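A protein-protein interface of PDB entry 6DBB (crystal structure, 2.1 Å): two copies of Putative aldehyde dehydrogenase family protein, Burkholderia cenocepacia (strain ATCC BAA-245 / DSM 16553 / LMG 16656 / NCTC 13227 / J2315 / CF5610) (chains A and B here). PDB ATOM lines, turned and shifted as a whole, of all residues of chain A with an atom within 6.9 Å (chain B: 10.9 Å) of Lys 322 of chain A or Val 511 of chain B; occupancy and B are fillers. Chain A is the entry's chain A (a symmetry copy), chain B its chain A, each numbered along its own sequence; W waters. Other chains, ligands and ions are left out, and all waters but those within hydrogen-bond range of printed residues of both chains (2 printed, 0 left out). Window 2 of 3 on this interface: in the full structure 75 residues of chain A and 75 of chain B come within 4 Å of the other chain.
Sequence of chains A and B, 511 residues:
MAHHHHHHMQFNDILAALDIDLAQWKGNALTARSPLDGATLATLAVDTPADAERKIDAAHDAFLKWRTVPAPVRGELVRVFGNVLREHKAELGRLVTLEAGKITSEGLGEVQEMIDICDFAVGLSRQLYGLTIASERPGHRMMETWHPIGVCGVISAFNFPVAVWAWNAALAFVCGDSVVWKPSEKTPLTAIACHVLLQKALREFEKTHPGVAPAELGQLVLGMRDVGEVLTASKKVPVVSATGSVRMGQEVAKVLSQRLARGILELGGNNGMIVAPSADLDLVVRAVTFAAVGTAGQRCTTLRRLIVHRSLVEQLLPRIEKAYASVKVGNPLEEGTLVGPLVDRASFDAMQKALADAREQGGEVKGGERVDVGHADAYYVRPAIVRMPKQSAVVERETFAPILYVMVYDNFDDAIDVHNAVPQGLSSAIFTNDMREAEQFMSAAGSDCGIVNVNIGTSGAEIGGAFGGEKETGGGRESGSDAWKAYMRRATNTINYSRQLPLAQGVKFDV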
ATOM      1  N   ASP A 282      -5.643  -7.789  36.885  1.00  0.00           N
ATOM      2  CA  ASP A 282      -6.443  -7.264  35.773  1.00  0.00           C
ATOM      3  C   ASP A 282      -6.661  -5.771  35.932  1.00  0.00           C
ATOM      4  O   ASP A 282      -6.576  -5.008  34.962  1.00  0.00           O
ATOM      5  CB  ASP A 282      -7.801  -7.967  35.692  1.00  0.00           C
ATOM      6  CG  ASP A 282      -7.680  -9.419  35.292  1.00  0.00           C
ATOM      7  OD1 ASP A 282      -6.725  -9.747  34.557  1.00  0.00           O
ATOM      8  OD2 ASP A 282      -8.549 -10.223  35.695  1.00  0.00           O
ATOM      9  N   VAL A 285      -2.964  -3.750  35.589  1.00  0.00           N
ATOM     10  CA  VAL A 285      -2.369  -3.547  34.269  1.00  0.00           C
ATOM     11  C   VAL A 285      -3.045  -2.377  33.559  1.00  0.00           C
ATOM     12  O   VAL A 285      -2.377  -1.548  32.927  1.00  0.00           O
ATOM     13  CB  VAL A 285      -2.413  -4.848  33.435  1.00  0.00           C
ATOM     14  CG1 VAL A 285      -3.838  -5.334  33.223  1.00  0.00           C
ATOM     15  CG2 VAL A 285      -1.721  -4.636  32.091  1.00  0.00           C
ATOM     16  N   LEU A 316       3.117  -9.846  36.031  1.00  0.00           N
ATOM     17  CA  LEU A 316       2.549  -8.535  35.730  1.00  0.00           C
ATOM     18  C   LEU A 316       3.289  -7.811  34.611  1.00  0.00           C
ATOM     19  O   LEU A 316       2.653  -7.234  33.719  1.00  0.00           O
ATOM     20  CB  LEU A 316       2.552  -7.685  36.997  1.00  0.00           C
ATOM     21  CG  LEU A 316       2.104  -6.239  36.869  1.00  0.00           C
ATOM     22  CD1 LEU A 316       0.668  -6.224  36.357  1.00  0.00           C
ATOM     23  CD2 LEU A 316       2.230  -5.553  38.230  1.00  0.00           C
ATOM     24  N   LEU A 317       4.617  -7.833  34.632  1.00  0.00           N
ATOM     25  CA  LEU A 317       5.369  -6.996  33.701  1.00  0.00           C
ATOM     26  C   LEU A 317       5.121  -7.340  32.233  1.00  0.00           C
ATOM     27  O   LEU A 317       4.961  -6.402  31.432  1.00  0.00           O
ATOM     28  CB  LEU A 317       6.868  -7.060  34.033  1.00  0.00           C
ATOM     29  CG  LEU A 317       7.361  -5.950  34.964  1.00  0.00           C
ATOM     30  CD1 LEU A 317       7.289  -4.582  34.279  1.00  0.00           C
ATOM     31  CD2 LEU A 317       6.589  -5.944  36.275  1.00  0.00           C
ATOM     32  N   PRO A 318       5.070  -8.610  31.809  1.00  0.00           N
ATOM     33  CA  PRO A 318       4.746  -8.871  30.397  1.00  0.00           C
ATOM     34  C   PRO A 318       3.371  -8.379  30.006  1.00  0.00           C
ATOM     35  O   PRO A 318       3.174  -8.004  28.843  1.00  0.00           O
ATOM     36  CB  PRO A 318       4.864 -10.398  30.281  1.00  0.00           C
ATOM     37  CG  PRO A 318       5.784 -10.776  31.363  1.00  0.00           C
ATOM     38  CD  PRO A 318       5.472  -9.849  32.497  1.00  0.00           C
ATOM     39  N   ARG A 319       2.410  -8.361  30.941  1.00  0.00           N
ATOM     40  CA  ARG A 319       1.090  -7.818  30.627  1.00  0.00           C
ATOM     41  C   ARG A 319       1.157  -6.313  30.399  1.00  0.00           C
ATOM     42  O   ARG A 319       0.527  -5.794  29.468  1.00  0.00           O
ATOM     43  CB  ARG A 319       0.089  -8.164  31.734  1.00  0.00           C
ATOM     44  CG  ARG A 319      -0.087  -9.675  31.941  1.00  0.00           C
ATOM     45  CD  ARG A 319      -1.261  -9.965  32.885  1.00  0.00           C
ATOM     46  NE  ARG A 319      -2.517  -9.442  32.345  1.00  0.00           N
ATOM     47  CZ  ARG A 319      -3.682  -9.469  32.986  1.00  0.00           C
ATOM     48  NH1 ARG A 319      -3.764 -10.004  34.197  1.00  0.00           N
ATOM     49  NH2 ARG A 319      -4.770  -8.976  32.412  1.00  0.00           N
ATOM     50  N   ILE A 320       1.927  -5.598  31.221  1.00  0.00           N
ATOM     51  CA  ILE A 320       2.087  -4.161  31.009  1.00  0.00           C
ATOM     52  C   ILE A 320       2.833  -3.892  29.704  1.00  0.00           C
ATOM     53  O   ILE A 320       2.464  -2.995  28.938  1.00  0.00           O
ATOM     54  CB  ILE A 320       2.803  -3.511  32.208  1.00  0.00           C
ATOM     55  CG1 ILE A 320       1.970  -3.668  33.487  1.00  0.00           C
ATOM     56  CG2 ILE A 320       3.086  -2.028  31.926  1.00  0.00           C
ATOM     57  CD1 ILE A 320       2.714  -3.254  34.740  1.00  0.00           C
ATOM     58  N   GLU A 321       3.885  -4.670  29.423  1.00  0.00           N
ATOM     59  CA  GLU A 321       4.614  -4.498  28.167  1.00  0.00           C
ATOM     60  C   GLU A 321       3.708  -4.754  26.971  1.00  0.00           C
ATOM     61  O   GLU A 321       3.764  -4.031  25.970  1.00  0.00           O
ATOM     62  CB  GLU A 321       5.832  -5.425  28.125  1.00  0.00           C
ATOM     63  CG  GLU A 321       6.898  -5.092  29.155  1.00  0.00           C
ATOM     64  CD  GLU A 321       7.991  -6.148  29.221  1.00  0.00           C
ATOM     65  OE1 GLU A 321       7.876  -7.172  28.523  1.00  0.00           O
ATOM     66  OE2 GLU A 321       8.957  -5.965  29.988  1.00  0.00           O
ATOM     67  N   LYS A 322       2.875  -5.790  27.058  1.00  0.00           N
ATOM     68  CA  LYS A 322       1.924  -6.077  25.991  1.00  0.00           C
ATOM     69  C   LYS A 322       0.969  -4.904  25.780  1.00  0.00           C
ATOM     70  O   LYS A 322       0.747  -4.467  24.644  1.00  0.00           O
ATOM     71  CB  LYS A 322       1.161  -7.358  26.325  1.00  0.00           C
ATOM     72  CG  LYS A 322       0.088  -7.714  25.324  1.00  0.00           C
ATOM     73  CD  LYS A 322      -0.720  -8.921  25.795  1.00  0.00           C
ATOM     74  CE  LYS A 322      -1.807  -9.265  24.775  1.00  0.00           C
ATOM     75  NZ  LYS A 322      -2.526 -10.526  25.097  1.00  0.00           N
ATOM     76  N   ALA A 323       0.407  -4.358  26.869  1.00  0.00           N
ATOM     77  CA  ALA A 323      -0.453  -3.180  26.734  1.00  0.00           C
ATOM     78  C   ALA A 323       0.314  -2.012  26.114  1.00  0.00           C
ATOM     79  O   ALA A 323      -0.169  -1.365  25.180  1.00  0.00           O
ATOM     80  CB  ALA A 323      -1.034  -2.777  28.094  1.00  0.00           C
ATOM     81  N   TYR A 324       1.514  -1.726  26.633  1.00  0.00           N
ATOM     82  CA  TYR A 324       2.339  -0.642  26.096  1.00  0.00           C
ATOM     83  C   TYR A 324       2.507  -0.756  24.582  1.00  0.00           C
ATOM     84  O   TYR A 324       2.300   0.217  23.845  1.00  0.00           O
ATOM     85  CB  TYR A 324       3.707  -0.639  26.786  1.00  0.00           C
ATOM     86  CG  TYR A 324       3.821   0.354  27.933  1.00  0.00           C
ATOM     87  CD1 TYR A 324       2.979   0.281  29.036  1.00  0.00           C
ATOM     88  CD2 TYR A 324       4.794   1.345  27.925  1.00  0.00           C
ATOM     89  CE1 TYR A 324       3.098   1.191  30.096  1.00  0.00           C
ATOM     90  CE2 TYR A 324       4.919   2.244  28.973  1.00  0.00           C
ATOM     91  CZ  TYR A 324       4.078   2.160  30.061  1.00  0.00           C
ATOM     92  OH  TYR A 324       4.223   3.073  31.089  1.00  0.00           O
ATOM     93  N   ALA A 325       2.890  -1.939  24.097  1.00  0.00           N
ATOM     94  CA  ALA A 325       3.164  -2.077  22.670  1.00  0.00           C
ATOM     95  C   ALA A 325       1.915  -1.840  21.834  1.00  0.00           C
ATOM     96  O   ALA A 325       2.014  -1.424  20.675  1.00  0.00           O
ATOM     97  CB  ALA A 325       3.745  -3.462  22.365  1.00  0.00           C
ATOM     98  N   SER A 326       0.738  -2.093  22.395  1.00  0.00           N
ATOM     99  CA  SER A 326      -0.490  -1.933  21.637  1.00  0.00           C
ATOM    100  C   SER A 326      -1.026  -0.512  21.679  1.00  0.00           C
ATOM    101  O   SER A 326      -1.996  -0.214  20.973  1.00  0.00           O
ATOM    102  CB  SER A 326      -1.561  -2.896  22.154  1.00  0.00           C
ATOM    103  OG  SER A 326      -2.090  -2.440  23.395  1.00  0.00           O
ATOM    104  N   VAL A 327      -0.421   0.370  22.477  1.00  0.00           N
ATOM    105  CA  VAL A 327      -0.914   1.738  22.583  1.00  0.00           C
ATOM    106  C   VAL A 327      -0.660   2.482  21.278  1.00  0.00           C
ATOM    107  O   VAL A 327       0.451   2.460  20.730  1.00  0.00           O
ATOM    108  CB  VAL A 327      -0.248   2.450  23.766  1.00  0.00           C
ATOM    109  CG1 VAL A 327      -0.372   3.935  23.597  1.00  0.00           C
ATOM    110  CG2 VAL A 327      -0.881   2.000  25.081  1.00  0.00           C
ATOM    111  N   LEU B 501     -13.408  -3.075  36.010  1.00  0.00           N
ATOM    112  CA  LEU B 501     -12.244  -2.734  35.198  1.00  0.00           C
ATOM    113  C   LEU B 501     -12.535  -1.509  34.341  1.00  0.00           C
ATOM    114  O   LEU B 501     -13.654  -1.351  33.843  1.00  0.00           O
ATOM    115  CB  LEU B 501     -11.853  -3.898  34.294  1.00  0.00           C
ATOM    116  CG  LEU B 501     -11.492  -5.170  35.061  1.00  0.00           C
ATOM    117  CD1 LEU B 501     -11.002  -6.255  34.116  1.00  0.00           C
ATOM    118  CD2 LEU B 501     -10.453  -4.850  36.114  1.00  0.00           C
ATOM    119  N   ALA B 504     -11.143  -0.738  27.979  1.00  0.00           N
ATOM    120  CA  ALA B 504      -9.857  -1.071  27.385  1.00  0.00           C
ATOM    121  C   ALA B 504      -9.348   0.036  26.463  1.00  0.00           C
ATOM    122  O   ALA B 504      -8.133   0.170  26.281  1.00  0.00           O
ATOM    123  CB  ALA B 504      -9.969  -2.397  26.627  1.00  0.00           C
ATOM    124  N   GLY B 506      -9.368   0.070  23.367  1.00  0.00           N
ATOM    125  CA  GLY B 506      -8.646  -0.583  22.289  1.00  0.00           C
ATOM    126  C   GLY B 506      -7.248  -1.047  22.635  1.00  0.00           C
ATOM    127  O   GLY B 506      -6.552  -1.570  21.761  1.00  0.00           O
ATOM    128  N   VAL B 507      -6.804  -0.845  23.857  1.00  0.00           N
ATOM    129  CA  VAL B 507      -5.530  -1.375  24.319  1.00  0.00           C
ATOM    130  C   VAL B 507      -5.688  -2.862  24.613  1.00  0.00           C
ATOM    131  O   VAL B 507      -6.739  -3.311  25.089  1.00  0.00           O
ATOM    132  CB  VAL B 507      -5.065  -0.584  25.559  1.00  0.00           C
ATOM    133  CG1 VAL B 507      -3.717  -1.089  26.069  1.00  0.00           C
ATOM    134  CG2 VAL B 507      -4.995   0.905  25.224  1.00  0.00           C
ATOM    135  N   LYS B 508      -4.642  -3.639  24.331  1.00  0.00           N
ATOM    136  CA  LYS B 508      -4.681  -5.094  24.503  1.00  0.00           C
ATOM    137  C   LYS B 508      -4.328  -5.456  25.943  1.00  0.00           C
ATOM    138  O   LYS B 508      -3.156  -5.467  26.329  1.00  0.00           O
ATOM    139  CB  LYS B 508      -3.748  -5.765  23.508  1.00  0.00           C
ATOM    140  CG  LYS B 508      -4.192  -5.541  22.084  1.00  0.00           C
ATOM    141  CD  LYS B 508      -3.193  -6.051  21.082  1.00  0.00           C
ATOM    142  CE  LYS B 508      -3.572  -5.570  19.692  1.00  0.00           C
ATOM    143  NZ  LYS B 508      -5.047  -5.675  19.500  1.00  0.00           N
ATOM    144  N   PHE B 509      -5.353  -5.751  26.745  1.00  0.00           N
ATOM    145  CA  PHE B 509      -5.155  -6.156  28.127  1.00  0.00           C
ATOM    146  C   PHE B 509      -5.427  -7.634  28.358  1.00  0.00           C
ATOM    147  O   PHE B 509      -5.209  -8.120  29.473  1.00  0.00           O
ATOM    148  CB  PHE B 509      -6.064  -5.342  29.057  1.00  0.00           C
ATOM    149  CG  PHE B 509      -5.724  -3.883  29.128  1.00  0.00           C
ATOM    150  CD1 PHE B 509      -4.517  -3.460  29.657  1.00  0.00           C
ATOM    151  CD2 PHE B 509      -6.629  -2.932  28.677  1.00  0.00           C
ATOM    152  CE1 PHE B 509      -4.213  -2.092  29.740  1.00  0.00           C
ATOM    153  CE2 PHE B 509      -6.337  -1.565  28.755  1.00  0.00           C
ATOM    154  CZ  PHE B 509      -5.125  -1.146  29.286  1.00  0.00           C
ATOM    155  N   ASP B 510      -5.904  -8.353  27.349  1.00  0.00           N
ATOM    156  CA  ASP B 510      -6.268  -9.746  27.541  1.00  0.00           C
ATOM    157  C   ASP B 510      -5.035 -10.595  27.815  1.00  0.00           C
ATOM    158  O   ASP B 510      -3.939 -10.327  27.314  1.00  0.00           O
ATOM    159  CB  ASP B 510      -7.022 -10.272  26.326  1.00  0.00           C
ATOM    160  CG  ASP B 510      -8.432  -9.725  26.244  1.00  0.00           C
ATOM    161  OD1 ASP B 510      -8.846  -8.995  27.179  1.00  0.00           O
ATOM    162  OD2 ASP B 510      -9.125 -10.037  25.252  1.00  0.00           O
ATOM    163  N   VAL B 511      -5.223 -11.637  28.614  1.00  0.00           N
ATOM    164  CA  VAL B 511      -4.128 -12.547  28.892  1.00  0.00           C
ATOM    165  C   VAL B 511      -4.051 -13.564  27.767  1.00  0.00           C
ATOM    166  O   VAL B 511      -2.965 -13.832  27.254  1.00  0.00           O
ATOM    167  CB  VAL B 511      -4.296 -13.226  30.266  1.00  0.00           C
ATOM    168  CG1 VAL B 511      -2.996 -13.872  30.702  1.00  0.00           C
ATOM    169  CG2 VAL B 511      -4.730 -12.207  31.291  1.00  0.00           C
ATOM    170  OXT VAL B 511      -5.064 -14.106  27.321  1.00  0.00           O
HETATM  171  O   HOH W   1      -2.291  -9.005  29.622  1.00  0.00           O
HETATM  172  O   HOH W   2      -1.765  -6.628  28.438  1.00  0.00           O
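The backbone NH (N) of Lys 508 of chain B lies within hydrogen-bond range of the side-chain hydroxyl (OG) of Ser 326 of chain A (3.0 Å).
O of Phe 509 of chain B is in hydrogen-bond range of NH2 of Arg 319 of chain A (3.1 Å).
The backbone carbonyl oxygen of Asp 510 of chain B sits at hydrogen-bond distance from the side-chain amino group of Lys 322 of chain A (2.6 Å).
NZ of Lys 322 of chain A lies within salt-bridge range of O of Val 511 of chain B (3.97 Å).
The guanidinium group of Arg 319 of chain A is in salt-bridge range of the side-chain carboxylate of Asp 282 of chain A (3.0 Å).
The backbone carbonyl oxygen of Ala 323 of chain A sits at hydrogen-bond distance from the side-chain hydroxyl of Ser 326 of chain A (2.8 Å).
Among the printed residues, pairs that only touch across the chains: Asp 282 of chain A with Leu 501 of chain B, Val 285 of chain A with Phe 509 of chain B, Arg 319 of chain A with Val 511 of chain B, Ala 323 of chain A with Val 507 of chain B, Ala 323 of chain A with Lys 508 of chain B, Ala 323 of chain A with Phe 509 of chain B and Ser 326 of chain A with Val 507 of chain B.
Of the printed residues of chain B, Asp 282 of chain A touches Leu 501 (3.9 Å).
No residue of chain B comes within 4 Å of Glu 321 of chain A.
Lys 322 of chain A touches just these residues of chain B: Asp 510 and Val 511.
Ala 323 of chain A touches just these residues of chain B: Val 507, Lys 508 and Phe 509.
Tyr 324 of chain A touches none of the printed residues of chain B.
No residue of chain B comes within 4 Å of Ala 325 of chain A.
Printed residues of chain A within 4 Å of Val 507 of chain B: Ala 323 (3.7 Å) and Ser 326 (3.4 Å).
Printed residues of chain A within 4 Å of Lys 508 of chain B: Ala 323 and Ser 326.
Of the printed residues of chain A, Phe 509 of chain B touches Val 285 (3.7 Å), Arg 319 (3.1 Å) and Ala 323 (3.6 Å).
Of the printed residues of chain A, Asp 510 of chain B touches Lys 322 (2.6 Å).
Val 511 of chain B touches just these residues of chain A: Arg 319 and Lys 322.
The nearest residue of chain B that does not touch Lys 322 of chain A is Lys 508 of chain B (4.1 Å).
The nearest residue of chain A that does not touch Val 511 of chain B is Asp 282 of chain A (4.5 Å).
The nearest printed residue of chain A that does not touch Lys 508 of chain B is Lys 322 of chain A (4.1 Å).
Hydrophobic or aromatic side chains of chain B that line the printed part of chain A: Leu 501, Val 507, Phe 509 and Val 511.
Of the 14 printed residues of chain A, 6 touch a printed residue of chain B.
Among the printed residues, no Asp or Glu carboxylate lies within 4 Å of a Lys or Arg side-chain nitrogen of the other chain.
No position is printed for both chains.
Of the 11 pairs that touch across the chains among the printed residues, none has its exchanged pair printed and touching as well.
Water W2 lies within hydrogen-bond range of the backbone carbonyl oxygen of Arg 319 of chain A (2.6 Å) and the backbone carbonyl oxygen of Lys 508 of chain B (2.8 Å).
Water W1 lies within hydrogen-bond range of NE of Arg 319 of chain A (2.8 Å), O of Phe 509 of chain B (3.1 Å) and O of Asp 510 of chain B (3.1 Å).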
